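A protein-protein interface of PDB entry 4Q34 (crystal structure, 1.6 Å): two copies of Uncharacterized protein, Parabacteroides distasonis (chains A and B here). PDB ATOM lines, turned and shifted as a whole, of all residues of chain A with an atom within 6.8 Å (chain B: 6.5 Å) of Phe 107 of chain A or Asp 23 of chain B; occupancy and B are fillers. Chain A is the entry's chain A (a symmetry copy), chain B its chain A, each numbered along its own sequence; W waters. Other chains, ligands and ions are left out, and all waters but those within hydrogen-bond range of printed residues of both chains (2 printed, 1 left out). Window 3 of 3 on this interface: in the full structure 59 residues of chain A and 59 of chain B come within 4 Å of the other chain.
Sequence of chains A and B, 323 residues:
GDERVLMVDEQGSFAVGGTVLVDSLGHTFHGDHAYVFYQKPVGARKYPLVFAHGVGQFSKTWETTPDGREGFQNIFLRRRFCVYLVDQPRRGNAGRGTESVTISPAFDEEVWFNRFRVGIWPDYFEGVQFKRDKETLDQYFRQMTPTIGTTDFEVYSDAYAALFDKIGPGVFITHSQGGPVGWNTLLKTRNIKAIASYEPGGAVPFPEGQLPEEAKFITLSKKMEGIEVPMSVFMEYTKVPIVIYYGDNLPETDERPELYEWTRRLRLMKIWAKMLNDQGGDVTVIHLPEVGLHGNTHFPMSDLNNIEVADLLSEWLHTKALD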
ATOM      1  N   SER A 104       6.476  20.283  -7.490  1.00  0.00           N
ATOM      2  CA  SER A 104       6.976  19.343  -8.489  1.00  0.00           C
ATOM      3  C   SER A 104       8.326  19.795  -8.995  1.00  0.00           C
ATOM      4  O   SER A 104       8.484  20.975  -9.297  1.00  0.00           O
ATOM      5  CB  SER A 104       6.050  19.318  -9.691  1.00  0.00           C
ATOM      6  OG  SER A 104       4.826  18.732  -9.338  1.00  0.00           O
ATOM      7  N   PRO A 105       9.281  18.867  -9.161  1.00  0.00           N
ATOM      8  CA  PRO A 105      10.553  19.276  -9.778  1.00  0.00           C
ATOM      9  C   PRO A 105      10.358  19.895 -11.162  1.00  0.00           C
ATOM     10  O   PRO A 105       9.551  19.383 -11.922  1.00  0.00           O
ATOM     11  CB  PRO A 105      11.301  17.958  -9.926  1.00  0.00           C
ATOM     12  CG  PRO A 105      10.789  17.146  -8.803  1.00  0.00           C
ATOM     13  CD  PRO A 105       9.320  17.455  -8.745  1.00  0.00           C
ATOM     14  N   ALA A 106      11.109  20.949 -11.465  1.00  0.00           N
ATOM     15  CA  ALA A 106      11.094  21.606 -12.763  1.00  0.00           C
ATOM     16  C   ALA A 106      12.482  21.510 -13.376  1.00  0.00           C
ATOM     17  O   ALA A 106      13.480  21.791 -12.707  1.00  0.00           O
ATOM     18  CB  ALA A 106      10.718  23.080 -12.583  1.00  0.00           C
ATOM     19  N   PHE A 107      12.544  21.153 -14.644  1.00  0.00           N
ATOM     20  CA  PHE A 107      13.816  21.003 -15.340  1.00  0.00           C
ATOM     21  C   PHE A 107      14.242  22.342 -15.952  1.00  0.00           C
ATOM     22  O   PHE A 107      14.267  22.514 -17.179  1.00  0.00           O
ATOM     23  CB  PHE A 107      13.726  19.894 -16.392  1.00  0.00           C
ATOM     24  CG  PHE A 107      13.654  18.528 -15.800  1.00  0.00           C
ATOM     25  CD1 PHE A 107      12.428  17.970 -15.436  1.00  0.00           C
ATOM     26  CD2 PHE A 107      14.819  17.807 -15.545  1.00  0.00           C
ATOM     27  CE1 PHE A 107      12.365  16.704 -14.858  1.00  0.00           C
ATOM     28  CE2 PHE A 107      14.759  16.538 -14.987  1.00  0.00           C
ATOM     29  CZ  PHE A 107      13.541  15.993 -14.635  1.00  0.00           C
ATOM     30  N   ASP A 108      14.595  23.264 -15.077  1.00  0.00           N
ATOM     31  CA  ASP A 108      15.019  24.591 -15.511  1.00  0.00           C
ATOM     32  C   ASP A 108      16.368  24.995 -14.931  1.00  0.00           C
ATOM     33  O   ASP A 108      16.696  26.176 -14.865  1.00  0.00           O
ATOM     34  CB  ASP A 108      13.967  25.633 -15.156  1.00  0.00           C
ATOM     35  CG  ASP A 108      13.684  25.688 -13.690  1.00  0.00           C
ATOM     36  OD1 ASP A 108      14.414  25.029 -12.915  1.00  0.00           O
ATOM     37  OD2 ASP A 108      12.728  26.383 -13.317  1.00  0.00           O
ATOM     38  N   GLU A 109      17.185  24.012 -14.564  1.00  0.00           N
ATOM     39  CA  GLU A 109      18.534  24.365 -14.038  1.00  0.00           C
ATOM     40  C   GLU A 109      19.411  25.157 -15.038  1.00  0.00           C
ATOM     41  O   GLU A 109      20.098  26.121 -14.659  1.00  0.00           O
ATOM     42  CB  GLU A 109      19.257  23.090 -13.597  1.00  0.00           C
ATOM     43  CG  GLU A 109      18.612  22.540 -12.332  1.00  0.00           C
ATOM     44  CD  GLU A 109      19.304  21.331 -11.738  1.00  0.00           C
ATOM     45  OE1 GLU A 109      20.158  20.668 -12.364  1.00  0.00           O
ATOM     46  OE2 GLU A 109      18.967  21.044 -10.583  1.00  0.00           O
ATOM     47  N   GLU A 110      19.351  24.746 -16.296  1.00  0.00           N
ATOM     48  CA  GLU A 110      20.066  25.437 -17.362  1.00  0.00           C
ATOM     49  C   GLU A 110      19.574  26.876 -17.590  1.00  0.00           C
ATOM     50  O   GLU A 110      20.350  27.777 -18.011  1.00  0.00           O
ATOM     51  CB  GLU A 110      20.021  24.602 -18.650  1.00  0.00           C
ATOM     52  CG  GLU A 110      20.636  23.207 -18.497  1.00  0.00           C
ATOM     53  CD  GLU A 110      19.721  22.150 -17.890  1.00  0.00           C
ATOM     54  OE1 GLU A 110      18.505  22.420 -17.646  1.00  0.00           O
ATOM     55  OE2 GLU A 110      20.225  21.007 -17.673  1.00  0.00           O
ATOM     56  N   VAL A 111      18.285  27.085 -17.381  1.00  0.00           N
ATOM     57  CA  VAL A 111      17.695  28.428 -17.422  1.00  0.00           C
ATOM     58  C   VAL A 111      18.199  29.282 -16.257  1.00  0.00           C
ATOM     59  O   VAL A 111      18.671  30.410 -16.464  1.00  0.00           O
ATOM     60  CB  VAL A 111      16.157  28.389 -17.456  1.00  0.00           C
ATOM     61  CG1 VAL A 111      15.603  29.803 -17.494  1.00  0.00           C
ATOM     62  CG2 VAL A 111      15.663  27.567 -18.646  1.00  0.00           C
ATOM     63  N   LEU B  21      18.069  13.780 -11.689  1.00  0.00           N
ATOM     64  CA  LEU B  21      17.107  13.331 -12.679  1.00  0.00           C
ATOM     65  C   LEU B  21      17.532  13.935 -13.988  1.00  0.00           C
ATOM     66  O   LEU B  21      18.133  15.002 -14.014  1.00  0.00           O
ATOM     67  CB  LEU B  21      15.711  13.776 -12.316  1.00  0.00           C
ATOM     68  CG  LEU B  21      15.197  13.557 -10.906  1.00  0.00           C
ATOM     69  CD1 LEU B  21      13.805  14.127 -10.808  1.00  0.00           C
ATOM     70  CD2 LEU B  21      15.164  12.080 -10.584  1.00  0.00           C
ATOM     71  N   VAL B  22      17.223  13.260 -15.106  1.00  0.00           N
ATOM     72  CA  VAL B  22      17.589  13.755 -16.426  1.00  0.00           C
ATOM     73  C   VAL B  22      16.385  13.567 -17.311  1.00  0.00           C
ATOM     74  O   VAL B  22      15.900  12.446 -17.458  1.00  0.00           O
ATOM     75  CB  VAL B  22      18.815  13.012 -17.034  1.00  0.00           C
ATOM     76  CG1 VAL B  22      19.226  13.629 -18.361  1.00  0.00           C
ATOM     77  CG2 VAL B  22      19.971  13.028 -16.063  1.00  0.00           C
ATOM     78  N   ASP B  23      15.899  14.648 -17.902  1.00  0.00           N
ATOM     79  CA  ASP B  23      14.688  14.564 -18.738  1.00  0.00           C
ATOM     80  C   ASP B  23      15.006  14.211 -20.184  1.00  0.00           C
ATOM     81  O   ASP B  23      16.173  14.087 -20.584  1.00  0.00           O
ATOM     82  CB  ASP B  23      13.807  15.829 -18.656  1.00  0.00           C
ATOM     83  CG  ASP B  23      14.375  17.019 -19.415  1.00  0.00           C
ATOM     84  OD1 ASP B  23      15.413  16.934 -20.124  1.00  0.00           O
ATOM     85  OD2 ASP B  23      13.763  18.082 -19.276  1.00  0.00           O
ATOM     86  N   SER B  24      13.938  14.076 -20.962  1.00  0.00           N
ATOM     87  CA  SER B  24      14.046  13.554 -22.311  1.00  0.00           C
ATOM     88  C   SER B  24      14.946  14.454 -23.147  1.00  0.00           C
ATOM     89  O   SER B  24      15.485  14.002 -24.137  1.00  0.00           O
ATOM     90  CB  SER B  24      12.648  13.419 -22.930  1.00  0.00           C
ATOM     91  OG  SER B  24      12.067  14.706 -23.136  1.00  0.00           O
ATOM     92  N   LEU B  25      15.128  15.712 -22.729  1.00  0.00           N
ATOM     93  CA  LEU B  25      15.980  16.675 -23.439  1.00  0.00           C
ATOM     94  C   LEU B  25      17.407  16.754 -22.883  1.00  0.00           C
ATOM     95  O   LEU B  25      18.212  17.542 -23.375  1.00  0.00           O
ATOM     96  CB  LEU B  25      15.342  18.077 -23.439  1.00  0.00           C
ATOM     97  CG  LEU B  25      13.886  18.190 -23.931  1.00  0.00           C
ATOM     98  CD1 LEU B  25      13.371  19.606 -23.699  1.00  0.00           C
ATOM     99  CD2 LEU B  25      13.729  17.793 -25.393  1.00  0.00           C
ATOM    100  N   GLY B  26      17.731  15.922 -21.892  1.00  0.00           N
ATOM    101  CA  GLY B  26      19.055  15.939 -21.268  1.00  0.00           C
ATOM    102  C   GLY B  26      19.227  17.016 -20.198  1.00  0.00           C
ATOM    103  O   GLY B  26      20.323  17.233 -19.700  1.00  0.00           O
ATOM    104  N   HIS B  27      18.133  17.649 -19.804  1.00  0.00           N
ATOM    105  CA  HIS B  27      18.199  18.684 -18.770  1.00  0.00           C
ATOM    106  C   HIS B  27      18.234  18.001 -17.402  1.00  0.00           C
ATOM    107  O   HIS B  27      17.660  16.925 -17.225  1.00  0.00           O
ATOM    108  CB  HIS B  27      17.016  19.643 -18.905  1.00  0.00           C
ATOM    109  CG  HIS B  27      17.100  20.520 -20.118  1.00  0.00           C
ATOM    110  ND1 HIS B  27      15.985  21.003 -20.773  1.00  0.00           N
ATOM    111  CD2 HIS B  27      18.171  20.969 -20.816  1.00  0.00           C
ATOM    112  CE1 HIS B  27      16.367  21.726 -21.811  1.00  0.00           C
ATOM    113  NE2 HIS B  27      17.690  21.734 -21.850  1.00  0.00           N
ATOM    114  N   THR B  28      18.886  18.635 -16.434  1.00  0.00           N
ATOM    115  CA  THR B  28      19.095  17.997 -15.125  1.00  0.00           C
ATOM    116  C   THR B  28      18.208  18.511 -14.022  1.00  0.00           C
ATOM    117  O   THR B  28      17.762  19.667 -14.028  1.00  0.00           O
ATOM    118  CB  THR B  28      20.565  18.153 -14.667  1.00  0.00           C
ATOM    119  OG1 THR B  28      20.934  19.551 -14.629  1.00  0.00           O
ATOM    120  CG2 THR B  28      21.449  17.411 -15.638  1.00  0.00           C
ATOM    121  N   PHE B  29      17.976  17.655 -13.043  1.00  0.00           N
ATOM    122  CA  PHE B  29      17.427  18.103 -11.790  1.00  0.00           C
ATOM    123  C   PHE B  29      18.166  17.459 -10.639  1.00  0.00           C
ATOM    124  O   PHE B  29      18.067  16.253 -10.414  1.00  0.00           O
ATOM    125  CB  PHE B  29      15.919  17.811 -11.715  1.00  0.00           C
ATOM    126  CG  PHE B  29      15.283  18.371 -10.494  1.00  0.00           C
ATOM    127  CD1 PHE B  29      15.296  17.632  -9.323  1.00  0.00           C
ATOM    128  CD2 PHE B  29      14.746  19.663 -10.492  1.00  0.00           C
ATOM    129  CE1 PHE B  29      14.730  18.113  -8.191  1.00  0.00           C
ATOM    130  CE2 PHE B  29      14.197  20.172  -9.293  1.00  0.00           C
ATOM    131  CZ  PHE B  29      14.179  19.377  -8.180  1.00  0.00           C
HETATM  132  O   HOH W   1      22.778  20.893 -16.060  1.00  0.00           O
HETATM  133  O   HOH W   2      21.902  19.577 -19.145  1.00  0.00           O
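Pro 105 of chain A touches Phe 29 of chain B (CB to CZ, 3.7 Å).
Phe 29 of chain B touches Ala 106 of chain A.
O of Leu 21 of chain B touches CE2 of Phe 107 of chain A, at 3.8 Å.
Phe 107 of chain A touches Asp 23 of chain B (CB to OD2, 3.4 Å).
CD2 of Phe 107 of chain A touches O of His 27 of chain B, 3.4 Å away.
C of Thr 28 of chain B touches CD2 of Phe 107 of chain A, 3.8 Å away.
CE2 of Phe 107 of chain A touches CB of Phe 29 of chain B, at 3.7 Å.
Glu 109 of chain A touches Phe 29 of chain B.
Glu 110 of chain A touches His 27 of chain B (OE2 to CA, 3.3 Å).
The backbone NH (N) of Thr 28 of chain B is in hydrogen-bond range of the side-chain carboxylate (OE2) of Glu 110 of chain A (3.0 Å).
OG1 of Thr 28 of chain B sits at hydrogen-bond distance from OE1 of Glu 109 of chain A, 2.6 Å away.
Of the 9 printed residues of chain B, 5 touch a printed residue of chain A.
Hydrophobic or aromatic side chains of chain B that line the printed part of chain A: Leu 21, His 27 and Phe 29.
Along chain B the printed residues that touch a printed residue of chain A span positions 21 to 29.
Among the printed residues, 11 pairs touch across the chains.
Water W2 lies within hydrogen-bond range of OE2 of Glu 110 of chain A and O of Gly 26 of chain B.
Water W1 bridges OG1 of Thr 28 of chain B (2.7 Å) and OE2 of Glu 110 of chain A (3.0 Å).
The side-chain carboxylate (OD1) of Asp 23 of chain B is in hydrogen-bond range of the backbone NH (N) of Leu 25 of chain B, 2.9 Å away.
N of Gly 26 of chain B is in hydrogen-bond range of OD1 of Asp 23 of chain B.
The side-chain carboxylate (OD1) of Asp 23 of chain B is in hydrogen-bond range of the backbone NH (N) of His 27 of chain B, at 2.8 Å.
The backbone carbonyl oxygen (O) of Phe 29 of chain B sits at hydrogen-bond distance from the backbone NH (N) of Leu 21 of chain B, 2.8 Å away.
No position is printed for both chains.
Of the 11 pairs that touch across the chains among the printed residues, none has its exchanged pair printed and touching as well.
Printed residues of chain B within 4 Å of Ala 106 of chain A: Phe 29 (3.3 Å).
Of chain B, only Leu 21 (3.8 Å), Asp 23 (3.4 Å), His 27 (3.4 Å), Thr 28 (3.8 Å) and Phe 29 (3.7 Å) come within 4 Å of Phe 107 of chain A.
Of the printed residues of chain B, Glu 110 of chain A touches His 27 and Thr 28.
Asp 23 of chain B touches just one residue of chain A: Phe 107 (3.4 Å).
Ser 24 of chain B touches none of the printed residues of chain A.
Leu 25 of chain B touches none of the printed residues of chain A.
Printed residues of chain A within 4 Å of Phe 29 of chain B: Pro 105 (3.7 Å), Ala 106 (3.3 Å), Phe 107 (3.7 Å) and Glu 109 (3.5 Å).
The nearest residue of chain B that does not touch Phe 107 of chain A is Val 22 of chain B (4.1 Å).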
